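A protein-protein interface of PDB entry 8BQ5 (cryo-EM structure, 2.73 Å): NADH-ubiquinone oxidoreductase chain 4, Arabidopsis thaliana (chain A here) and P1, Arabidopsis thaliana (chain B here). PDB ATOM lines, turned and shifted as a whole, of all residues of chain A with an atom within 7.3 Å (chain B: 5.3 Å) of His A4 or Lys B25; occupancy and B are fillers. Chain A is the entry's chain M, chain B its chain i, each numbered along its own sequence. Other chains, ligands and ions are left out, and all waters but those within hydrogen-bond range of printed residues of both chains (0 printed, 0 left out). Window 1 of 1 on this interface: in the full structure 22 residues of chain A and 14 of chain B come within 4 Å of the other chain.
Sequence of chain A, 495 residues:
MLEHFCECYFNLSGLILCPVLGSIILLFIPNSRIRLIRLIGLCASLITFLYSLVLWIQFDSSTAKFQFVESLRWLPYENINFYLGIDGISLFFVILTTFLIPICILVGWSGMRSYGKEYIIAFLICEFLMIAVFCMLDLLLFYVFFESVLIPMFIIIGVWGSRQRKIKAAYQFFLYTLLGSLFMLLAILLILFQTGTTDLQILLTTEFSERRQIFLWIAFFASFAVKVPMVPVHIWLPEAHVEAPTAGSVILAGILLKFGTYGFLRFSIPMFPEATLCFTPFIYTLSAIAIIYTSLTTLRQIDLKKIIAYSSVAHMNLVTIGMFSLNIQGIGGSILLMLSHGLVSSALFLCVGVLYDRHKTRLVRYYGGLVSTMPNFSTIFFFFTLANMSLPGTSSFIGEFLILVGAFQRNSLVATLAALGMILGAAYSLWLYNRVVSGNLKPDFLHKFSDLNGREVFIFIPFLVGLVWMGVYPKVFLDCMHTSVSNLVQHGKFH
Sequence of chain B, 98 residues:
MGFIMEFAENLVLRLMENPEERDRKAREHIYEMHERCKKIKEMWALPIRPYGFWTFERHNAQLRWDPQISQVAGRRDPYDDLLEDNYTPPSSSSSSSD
The backbone carbonyl oxygen (O) of Leu A2 is in hydrogen-bond range of the side-chain amide nitrogen (ND2) of Asn A81. O of Leu A2 lies within hydrogen-bond range of OH of Tyr A83, at 3.3 Å. O of His A4 sits close to O of Val A69 (2.7 Å). OG of Ser A71 sits at hydrogen-bond distance from N of His A4, at 3.0 Å. NH1 of Arg B22 lies within salt-bridge range of OD1 of Asp B23 (3.2 Å).
Of the printed residues of chain B, His A4 touches Lys B25. Of the printed residues of chain B, Phe A5 touches Lys B25. Of the printed residues of chain A, Asp B23 touches Lys A65. Of the printed residues of chain B, Lys A65 touches Asp B23 and Ala B26. The nearest residue of chain B that does not touch His A4 is Ala B26 (4.2 Å). The nearest residue of chain A that does not touch Lys B25 is Cys A6 (4.5 Å). The nearest printed residue of chain B that does not touch Glu A7 is Arg B24 (6.6 Å).
OE1 of Glu A7 lies within salt-bridge range of NZ of Lys B25, at 3.9 Å. NZ of Lys A65 is in salt-bridge range of OD1 of Asp B23, at 3.8 Å. The side-chain hydroxyl of Tyr A83 is in hydrogen-bond range of a ring nitrogen (ND1) of His B29 (3.3 Å). NE2 of Gln A201 sits at hydrogen-bond distance from NE2 of His B29 (3.4 Å).
Printed residues of chain B that touch a printed residue of chain A: Glu B21, Arg B22, Asp B23, Lys B25, Ala B26 and His B29. Among the printed residues, Asp or Glu carboxylates within 4 Å of a Lys or Arg side-chain nitrogen of the other chain: Glu A7 with Lys B25 and Lys A65 with Asp B23.
Among the printed residues, merely in contact across the chains: Leu A2 with His B29 (3.9 Å), His A4 with Lys B25 (3.2 Å), Phe A5 with Lys B25 (3.7 Å), Glu A7 with Glu B21 (3.8 Å), Lys A65 with Ala B26 (3.9 Å) and Phe A66 with Arg B22 (3.9 Å).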
ATOM      1  N   LEU A   2      18.737  16.547 -13.155  1.00  0.00           N
ATOM      2  CA  LEU A   2      18.534  16.953 -11.769  1.00  0.00           C
ATOM      3  C   LEU A   2      18.244  15.737 -10.897  1.00  0.00           C
ATOM      4  O   LEU A   2      17.178  15.134 -11.003  1.00  0.00           O
ATOM      5  CB  LEU A   2      17.386  17.958 -11.665  1.00  0.00           C
ATOM      6  CG  LEU A   2      17.264  18.751 -10.363  1.00  0.00           C
ATOM      7  CD1 LEU A   2      18.409  19.746 -10.219  1.00  0.00           C
ATOM      8  CD2 LEU A   2      15.913  19.450 -10.274  1.00  0.00           C
ATOM      9  N   GLU A   3      19.194  15.374 -10.037  1.00  0.00           N
ATOM     10  CA  GLU A   3      19.021  14.218  -9.163  1.00  0.00           C
ATOM     11  C   GLU A   3      18.085  14.591  -8.021  1.00  0.00           C
ATOM     12  O   GLU A   3      18.295  15.596  -7.334  1.00  0.00           O
ATOM     13  CB  GLU A   3      20.368  13.726  -8.646  1.00  0.00           C
ATOM     14  CG  GLU A   3      21.434  13.630  -9.725  1.00  0.00           C
ATOM     15  CD  GLU A   3      21.090  12.604 -10.795  1.00  0.00           C
ATOM     16  OE1 GLU A   3      20.315  11.668 -10.505  1.00  0.00           O
ATOM     17  OE2 GLU A   3      21.597  12.738 -11.928  1.00  0.00           O
ATOM     18  N   HIS A   4      17.050  13.777  -7.818  1.00  0.00           N
ATOM     19  CA  HIS A   4      16.017  14.032  -6.824  1.00  0.00           C
ATOM     20  C   HIS A   4      16.018  12.988  -5.715  1.00  0.00           C
ATOM     21  O   HIS A   4      14.967  12.707  -5.133  1.00  0.00           O
ATOM     22  CB  HIS A   4      14.646  14.081  -7.503  1.00  0.00           C
ATOM     23  CG  HIS A   4      13.673  15.008  -6.847  1.00  0.00           C
ATOM     24  ND1 HIS A   4      12.778  15.773  -7.564  1.00  0.00           N
ATOM     25  CD2 HIS A   4      13.449  15.291  -5.542  1.00  0.00           C
ATOM     26  CE1 HIS A   4      12.045  16.487  -6.729  1.00  0.00           C
ATOM     27  NE2 HIS A   4      12.432  16.214  -5.496  1.00  0.00           N
ATOM     28  N   PHE A   5      17.180  12.407  -5.412  1.00  0.00           N
ATOM     29  CA  PHE A   5      17.232  11.278  -4.492  1.00  0.00           C
ATOM     30  C   PHE A   5      16.703  11.674  -3.120  1.00  0.00           C
ATOM     31  O   PHE A   5      17.083  12.710  -2.565  1.00  0.00           O
ATOM     32  CB  PHE A   5      18.663  10.743  -4.376  1.00  0.00           C
ATOM     33  CG  PHE A   5      19.642  11.723  -3.787  1.00  0.00           C
ATOM     34  CD1 PHE A   5      20.161  12.760  -4.546  1.00  0.00           C
ATOM     35  CD2 PHE A   5      20.045  11.602  -2.466  1.00  0.00           C
ATOM     36  CE1 PHE A   5      21.062  13.656  -3.997  1.00  0.00           C
ATOM     37  CE2 PHE A   5      20.944  12.492  -1.915  1.00  0.00           C
ATOM     38  CZ  PHE A   5      21.453  13.519  -2.681  1.00  0.00           C
ATOM     39  N   CYS A   6      15.819  10.843  -2.576  1.00  0.00           N
ATOM     40  CA  CYS A   6      15.183  11.119  -1.299  1.00  0.00           C
ATOM     41  C   CYS A   6      16.126  10.782  -0.143  1.00  0.00           C
ATOM     42  O   CYS A   6      16.989   9.904  -0.237  1.00  0.00           O
ATOM     43  CB  CYS A   6      13.878  10.334  -1.175  1.00  0.00           C
ATOM     44  SG  CYS A   6      12.967  10.615   0.357  1.00  0.00           S
ATOM     45  N   GLU A   7      15.951  11.506   0.962  1.00  0.00           N
ATOM     46  CA  GLU A   7      16.768  11.317   2.153  1.00  0.00           C
ATOM     47  C   GLU A   7      16.298  10.165   3.026  1.00  0.00           C
ATOM     48  O   GLU A   7      17.047   9.728   3.907  1.00  0.00           O
ATOM     49  CB  GLU A   7      16.774  12.599   2.993  1.00  0.00           C
ATOM     50  CG  GLU A   7      16.799  13.875   2.170  1.00  0.00           C
ATOM     51  CD  GLU A   7      18.181  14.487   2.081  1.00  0.00           C
ATOM     52  OE1 GLU A   7      18.447  15.213   1.100  1.00  0.00           O
ATOM     53  OE2 GLU A   7      19.000  14.242   2.991  1.00  0.00           O
ATOM     54  N   CYS A   8      15.082   9.674   2.805  1.00  0.00           N
ATOM     55  CA  CYS A   8      14.509   8.634   3.644  1.00  0.00           C
ATOM     56  C   CYS A   8      15.231   7.309   3.437  1.00  0.00           C
ATOM     57  O   CYS A   8      15.603   6.946   2.318  1.00  0.00           O
ATOM     58  CB  CYS A   8      13.024   8.467   3.327  1.00  0.00           C
ATOM     59  SG  CYS A   8      11.972   9.761   4.011  1.00  0.00           S
ATOM     60  N   LYS A  65       2.660  17.949  -2.349  1.00  0.00           N
ATOM     61  CA  LYS A  65       3.835  17.663  -3.202  1.00  0.00           C
ATOM     62  C   LYS A  65       4.060  16.150  -3.206  1.00  0.00           C
ATOM     63  O   LYS A  65       3.786  15.500  -2.176  1.00  0.00           O
ATOM     64  CB  LYS A  65       5.047  18.447  -2.688  1.00  0.00           C
ATOM     65  CG  LYS A  65       5.228  19.831  -3.291  1.00  0.00           C
ATOM     66  CD  LYS A  65       4.528  20.922  -2.509  1.00  0.00           C
ATOM     67  CE  LYS A  65       4.885  22.312  -2.992  1.00  0.00           C
ATOM     68  NZ  LYS A  65       6.348  22.499  -3.120  1.00  0.00           N
ATOM     69  N   PHE A  66       4.519  15.618  -4.334  1.00  0.00           N
ATOM     70  CA  PHE A  66       4.784  14.163  -4.427  1.00  0.00           C
ATOM     71  C   PHE A  66       5.808  13.807  -3.354  1.00  0.00           C
ATOM     72  O   PHE A  66       6.790  14.550  -3.166  1.00  0.00           O
ATOM     73  CB  PHE A  66       5.140  13.792  -5.868  1.00  0.00           C
ATOM     74  CG  PHE A  66       3.957  13.851  -6.798  1.00  0.00           C
ATOM     75  CD1 PHE A  66       2.902  12.967  -6.653  1.00  0.00           C
ATOM     76  CD2 PHE A  66       3.883  14.809  -7.794  1.00  0.00           C
ATOM     77  CE1 PHE A  66       1.809  13.027  -7.501  1.00  0.00           C
ATOM     78  CE2 PHE A  66       2.788  14.869  -8.640  1.00  0.00           C
ATOM     79  CZ  PHE A  66       1.751  13.980  -8.490  1.00  0.00           C
ATOM     80  N   PHE A  68       8.464  11.110  -1.094  1.00  0.00           N
ATOM     81  CA  PHE A  68       9.509  10.123  -1.362  1.00  0.00           C
ATOM     82  C   PHE A  68       9.970  10.183  -2.810  1.00  0.00           C
ATOM     83  O   PHE A  68      10.322   9.158  -3.400  1.00  0.00           O
ATOM     84  CB  PHE A  68       9.044   8.706  -1.007  1.00  0.00           C
ATOM     85  CG  PHE A  68       8.252   8.634   0.263  1.00  0.00           C
ATOM     86  CD1 PHE A  68       8.710   9.246   1.417  1.00  0.00           C
ATOM     87  CD2 PHE A  68       7.040   7.971   0.299  1.00  0.00           C
ATOM     88  CE1 PHE A  68       7.977   9.189   2.583  1.00  0.00           C
ATOM     89  CE2 PHE A  68       6.303   7.911   1.462  1.00  0.00           C
ATOM     90  CZ  PHE A  68       6.773   8.520   2.605  1.00  0.00           C
ATOM     91  N   VAL A  69       9.962  11.383  -3.396  1.00  0.00           N
ATOM     92  CA  VAL A  69      10.304  11.518  -4.802  1.00  0.00           C
ATOM     93  C   VAL A  69      11.770  11.182  -4.993  1.00  0.00           C
ATOM     94  O   VAL A  69      12.641  11.662  -4.257  1.00  0.00           O
ATOM     95  CB  VAL A  69       9.982  12.928  -5.315  1.00  0.00           C
ATOM     96  CG1 VAL A  69      10.717  13.193  -6.618  1.00  0.00           C
ATOM     97  CG2 VAL A  69       8.501  13.076  -5.523  1.00  0.00           C
ATOM     98  N   GLU A  70      12.046  10.337  -5.978  1.00  0.00           N
ATOM     99  CA  GLU A  70      13.394   9.923  -6.310  1.00  0.00           C
ATOM    100  C   GLU A  70      13.465   9.699  -7.812  1.00  0.00           C
ATOM    101  O   GLU A  70      12.480   9.324  -8.453  1.00  0.00           O
ATOM    102  CB  GLU A  70      13.784   8.671  -5.519  1.00  0.00           C
ATOM    103  CG  GLU A  70      13.296   7.385  -6.131  1.00  0.00           C
ATOM    104  CD  GLU A  70      13.568   6.198  -5.247  1.00  0.00           C
ATOM    105  OE1 GLU A  70      13.329   5.060  -5.697  1.00  0.00           O
ATOM    106  OE2 GLU A  70      14.030   6.396  -4.104  1.00  0.00           O
ATOM    107  N   SER A  71      14.637   9.960  -8.377  1.00  0.00           N
ATOM    108  CA  SER A  71      14.804   9.962  -9.819  1.00  0.00           C
ATOM    109  C   SER A  71      15.746   8.848 -10.249  1.00  0.00           C
ATOM    110  O   SER A  71      16.599   8.389  -9.484  1.00  0.00           O
ATOM    111  CB  SER A  71      15.338  11.309 -10.320  1.00  0.00           C
ATOM    112  OG  SER A  71      16.634  11.561  -9.813  1.00  0.00           O
ATOM    113  N   LEU A  72      15.567   8.413 -11.493  1.00  0.00           N
ATOM    114  CA  LEU A  72      16.422   7.402 -12.098  1.00  0.00           C
ATOM    115  C   LEU A  72      16.798   7.874 -13.494  1.00  0.00           C
ATOM    116  O   LEU A  72      15.929   8.275 -14.273  1.00  0.00           O
ATOM    117  CB  LEU A  72      15.723   6.031 -12.110  1.00  0.00           C
ATOM    118  CG  LEU A  72      14.275   5.836 -12.580  1.00  0.00           C
ATOM    119  CD1 LEU A  72      14.153   5.861 -14.085  1.00  0.00           C
ATOM    120  CD2 LEU A  72      13.680   4.551 -12.021  1.00  0.00           C
ATOM    121  N   ASN A  81      14.856  12.082 -18.150  1.00  0.00           N
ATOM    122  CA  ASN A  81      15.047  11.653 -16.772  1.00  0.00           C
ATOM    123  C   ASN A  81      13.682  11.354 -16.171  1.00  0.00           C
ATOM    124  O   ASN A  81      12.708  12.057 -16.452  1.00  0.00           O
ATOM    125  CB  ASN A  81      15.782  12.723 -15.954  1.00  0.00           C
ATOM    126  CG  ASN A  81      16.356  12.180 -14.663  1.00  0.00           C
ATOM    127  OD1 ASN A  81      16.375  10.973 -14.441  1.00  0.00           O
ATOM    128  ND2 ASN A  81      16.841  13.073 -13.809  1.00  0.00           N
ATOM    129  N   PHE A  82      13.613  10.309 -15.348  1.00  0.00           N
ATOM    130  CA  PHE A  82      12.348   9.782 -14.857  1.00  0.00           C
ATOM    131  C   PHE A  82      12.298   9.831 -13.336  1.00  0.00           C
ATOM    132  O   PHE A  82      13.333   9.817 -12.665  1.00  0.00           O
ATOM    133  CB  PHE A  82      12.138   8.346 -15.322  1.00  0.00           C
ATOM    134  CG  PHE A  82      11.966   8.203 -16.802  1.00  0.00           C
ATOM    135  CD1 PHE A  82      10.918   8.828 -17.455  1.00  0.00           C
ATOM    136  CD2 PHE A  82      12.853   7.441 -17.543  1.00  0.00           C
ATOM    137  CE1 PHE A  82      10.756   8.697 -18.817  1.00  0.00           C
ATOM    138  CE2 PHE A  82      12.697   7.308 -18.905  1.00  0.00           C
ATOM    139  CZ  PHE A  82      11.642   7.930 -19.543  1.00  0.00           C
ATOM    140  N   TYR A  83      11.080   9.869 -12.797  1.00  0.00           N
ATOM    141  CA  TYR A  83      10.860  10.080 -11.372  1.00  0.00           C
ATOM    142  C   TYR A  83       9.871   9.074 -10.801  1.00  0.00           C
ATOM    143  O   TYR A  83       8.943   8.635 -11.487  1.00  0.00           O
ATOM    144  CB  TYR A  83      10.359  11.502 -11.104  1.00  0.00           C
ATOM    145  CG  TYR A  83      11.371  12.557 -11.467  1.00  0.00           C
ATOM    146  CD1 TYR A  83      11.532  12.973 -12.781  1.00  0.00           C
ATOM    147  CD2 TYR A  83      12.190  13.114 -10.497  1.00  0.00           C
ATOM    148  CE1 TYR A  83      12.471  13.925 -13.115  1.00  0.00           C
ATOM    149  CE2 TYR A  83      13.128  14.068 -10.820  1.00  0.00           C
ATOM    150  CZ  TYR A  83      13.265  14.471 -12.130  1.00  0.00           C
ATOM    151  OH  TYR A  83      14.201  15.424 -12.454  1.00  0.00           O
ATOM    152  N   LEU A  84      10.084   8.725  -9.533  1.00  0.00           N
ATOM    153  CA  LEU A  84       9.185   7.894  -8.748  1.00  0.00           C
ATOM    154  C   LEU A  84       8.663   8.697  -7.567  1.00  0.00           C
ATOM    155  O   LEU A  84       9.427   9.373  -6.875  1.00  0.00           O
ATOM    156  CB  LEU A  84       9.886   6.642  -8.211  1.00  0.00           C
ATOM    157  CG  LEU A  84      10.495   5.647  -9.190  1.00  0.00           C
ATOM    158  CD1 LEU A  84      10.839   4.360  -8.462  1.00  0.00           C
ATOM    159  CD2 LEU A  84       9.533   5.376 -10.319  1.00  0.00           C
ATOM    160  N   GLN A 201       4.779  16.116 -13.261  1.00  0.00           N
ATOM    161  CA  GLN A 201       4.873  17.388 -12.551  1.00  0.00           C
ATOM    162  C   GLN A 201       4.920  18.561 -13.518  1.00  0.00           C
ATOM    163  O   GLN A 201       4.487  19.669 -13.181  1.00  0.00           O
ATOM    164  CB  GLN A 201       6.103  17.395 -11.648  1.00  0.00           C
ATOM    165  CG  GLN A 201       5.946  16.578 -10.388  1.00  0.00           C
ATOM    166  CD  GLN A 201       7.258  15.996  -9.920  1.00  0.00           C
ATOM    167  OE1 GLN A 201       7.645  16.160  -8.764  1.00  0.00           O
ATOM    168  NE2 GLN A 201       7.949  15.301 -10.815  1.00  0.00           N
ATOM    169  N   GLU B  20      10.813  21.320   4.287  1.00  0.00           N
ATOM    170  CA  GLU B  20      11.463  22.408   3.502  1.00  0.00           C
ATOM    171  C   GLU B  20      12.312  21.823   2.374  1.00  0.00           C
ATOM    172  O   GLU B  20      12.235  22.342   1.249  1.00  0.00           O
ATOM    173  CB  GLU B  20      12.333  23.265   4.421  1.00  0.00           C
ATOM    174  CG  GLU B  20      11.643  23.631   5.721  1.00  0.00           C
ATOM    175  CD  GLU B  20      10.389  24.472   5.558  1.00  0.00           C
ATOM    176  OE1 GLU B  20       9.459  24.299   6.367  1.00  0.00           O
ATOM    177  OE2 GLU B  20      10.350  25.307   4.631  1.00  0.00           O
ATOM    178  N   GLU B  21      13.091  20.788   2.676  1.00  0.00           N
ATOM    179  CA  GLU B  21      13.974  20.168   1.655  1.00  0.00           C
ATOM    180  C   GLU B  21      13.097  19.620   0.531  1.00  0.00           C
ATOM    181  O   GLU B  21      13.439  19.867  -0.642  1.00  0.00           O
ATOM    182  CB  GLU B  21      14.824  19.094   2.324  1.00  0.00           C
ATOM    183  CG  GLU B  21      15.822  19.669   3.312  1.00  0.00           C
ATOM    184  CD  GLU B  21      16.609  18.661   4.133  1.00  0.00           C
ATOM    185  OE1 GLU B  21      16.609  17.466   3.766  1.00  0.00           O
ATOM    186  OE2 GLU B  21      17.222  19.078   5.138  1.00  0.00           O
ATOM    187  N   ARG B  22      11.998  18.947   0.879  1.00  0.00           N
ATOM    188  CA  ARG B  22      11.077  18.379  -0.138  1.00  0.00           C
ATOM    189  C   ARG B  22      10.497  19.501  -1.003  1.00  0.00           C
ATOM    190  O   ARG B  22      10.656  19.430  -2.232  1.00  0.00           O
ATOM    191  CB  ARG B  22       9.936  17.625   0.542  1.00  0.00           C
ATOM    192  CG  ARG B  22       9.155  16.704  -0.385  1.00  0.00           C
ATOM    193  CD  ARG B  22       7.675  16.651  -0.059  1.00  0.00           C
ATOM    194  NE  ARG B  22       7.430  16.201   1.304  1.00  0.00           N
ATOM    195  CZ  ARG B  22       6.942  16.961   2.276  1.00  0.00           C
ATOM    196  NH1 ARG B  22       6.639  18.227   2.039  1.00  0.00           N
ATOM    197  NH2 ARG B  22       6.763  16.456   3.483  1.00  0.00           N
ATOM    198  N   ASP B  23       9.861  20.491  -0.377  1.00  0.00           N
ATOM    199  CA  ASP B  23       9.186  21.584  -1.126  1.00  0.00           C
ATOM    200  C   ASP B  23      10.156  22.299  -2.070  1.00  0.00           C
ATOM    201  O   ASP B  23       9.710  22.696  -3.139  1.00  0.00           O
ATOM    202  CB  ASP B  23       8.492  22.555  -0.168  1.00  0.00           C
ATOM    203  CG  ASP B  23       7.386  21.897   0.643  1.00  0.00           C
ATOM    204  OD1 ASP B  23       6.921  20.811   0.235  1.00  0.00           O
ATOM    205  OD2 ASP B  23       6.998  22.475   1.677  1.00  0.00           O
ATOM    206  N   ARG B  24      11.420  22.453  -1.675  1.00  0.00           N
ATOM    207  CA  ARG B  24      12.412  23.184  -2.510  1.00  0.00           C
ATOM    208  C   ARG B  24      12.767  22.362  -3.758  1.00  0.00           C
ATOM    209  O   ARG B  24      12.790  22.957  -4.847  1.00  0.00           O
ATOM    210  CB  ARG B  24      13.636  23.526  -1.659  1.00  0.00           C
ATOM    211  CG  ARG B  24      14.736  24.264  -2.407  1.00  0.00           C
ATOM    212  CD  ARG B  24      16.061  24.158  -1.676  1.00  0.00           C
ATOM    213  NE  ARG B  24      16.489  22.776  -1.505  1.00  0.00           N
ATOM    214  CZ  ARG B  24      17.248  22.109  -2.365  1.00  0.00           C
ATOM    215  NH1 ARG B  24      17.675  22.700  -3.467  1.00  0.00           N
ATOM    216  NH2 ARG B  24      17.584  20.856  -2.118  1.00  0.00           N
ATOM    217  N   LYS B  25      13.013  21.056  -3.611  1.00  0.00           N
ATOM    218  CA  LYS B  25      13.409  20.190  -4.760  1.00  0.00           C
ATOM    219  C   LYS B  25      12.273  20.127  -5.780  1.00  0.00           C
ATOM    220  O   LYS B  25      12.565  19.927  -6.969  1.00  0.00           O
ATOM    221  CB  LYS B  25      13.796  18.802  -4.250  1.00  0.00           C
ATOM    222  CG  LYS B  25      15.090  18.756  -3.448  1.00  0.00           C
ATOM    223  CD  LYS B  25      15.514  17.367  -3.024  1.00  0.00           C
ATOM    224  CE  LYS B  25      14.638  16.770  -1.944  1.00  0.00           C
ATOM    225  NZ  LYS B  25      15.316  15.652  -1.245  1.00  0.00           N
ATOM    226  N   ALA B  26      11.040  20.334  -5.295  1.00  0.00           N
ATOM    227  CA  ALA B  26       9.843  20.313  -6.159  1.00  0.00           C
ATOM    228  C   ALA B  26       9.820  21.569  -7.026  1.00  0.00           C
ATOM    229  O   ALA B  26       9.462  21.449  -8.207  1.00  0.00           O
ATOM    230  CB  ALA B  26       8.619  20.221  -5.289  1.00  0.00           C
ATOM    231  N   ARG B  27      10.202  22.717  -6.458  1.00  0.00           N
ATOM    232  CA  ARG B  27      10.236  23.967  -7.217  1.00  0.00           C
ATOM    233  C   ARG B  27      11.408  24.011  -8.193  1.00  0.00           C
ATOM    234  O   ARG B  27      11.257  24.483  -9.329  1.00  0.00           O
ATOM    235  CB  ARG B  27      10.282  25.153  -6.261  1.00  0.00           C
ATOM    236  CG  ARG B  27       9.233  25.067  -5.185  1.00  0.00           C
ATOM    237  CD  ARG B  27       9.021  26.389  -4.500  1.00  0.00           C
ATOM    238  NE  ARG B  27       9.874  26.506  -3.326  1.00  0.00           N
ATOM    239  CZ  ARG B  27       9.437  26.416  -2.078  1.00  0.00           C
ATOM    240  NH1 ARG B  27       8.163  26.181  -1.808  1.00  0.00           N
ATOM    241  NH2 ARG B  27      10.300  26.551  -1.076  1.00  0.00           N
ATOM    242  N   GLU B  28      12.590  23.560  -7.758  1.00  0.00           N
ATOM    243  CA  GLU B  28      13.727  23.479  -8.669  1.00  0.00           C
ATOM    244  C   GLU B  28      13.365  22.671  -9.901  1.00  0.00           C
ATOM    245  O   GLU B  28      13.718  23.042 -11.027  1.00  0.00           O
ATOM    246  CB  GLU B  28      14.933  22.843  -7.974  1.00  0.00           C
ATOM    247  CG  GLU B  28      15.808  23.799  -7.187  1.00  0.00           C
ATOM    248  CD  GLU B  28      17.143  23.178  -6.810  1.00  0.00           C
ATOM    249  OE1 GLU B  28      17.145  22.072  -6.234  1.00  0.00           O
ATOM    250  OE2 GLU B  28      18.190  23.800  -7.088  1.00  0.00           O
ATOM    251  N   HIS B  29      12.644  21.570  -9.700  1.00  0.00           N
ATOM    252  CA  HIS B  29      12.287  20.684 -10.799  1.00  0.00           C
ATOM    253  C   HIS B  29      11.446  21.412 -11.843  1.00  0.00           C
ATOM    254  O   HIS B  29      11.765  21.396 -13.040  1.00  0.00           O
ATOM    255  CB  HIS B  29      11.552  19.475 -10.220  1.00  0.00           C
ATOM    256  CG  HIS B  29      11.011  18.535 -11.246  1.00  0.00           C
ATOM    257  ND1 HIS B  29      11.666  17.377 -11.598  1.00  0.00           N
ATOM    258  CD2 HIS B  29       9.863  18.553 -11.961  1.00  0.00           C
ATOM    259  CE1 HIS B  29      10.958  16.735 -12.507  1.00  0.00           C
ATOM    260  NE2 HIS B  29       9.857  17.425 -12.744  1.00  0.00           N
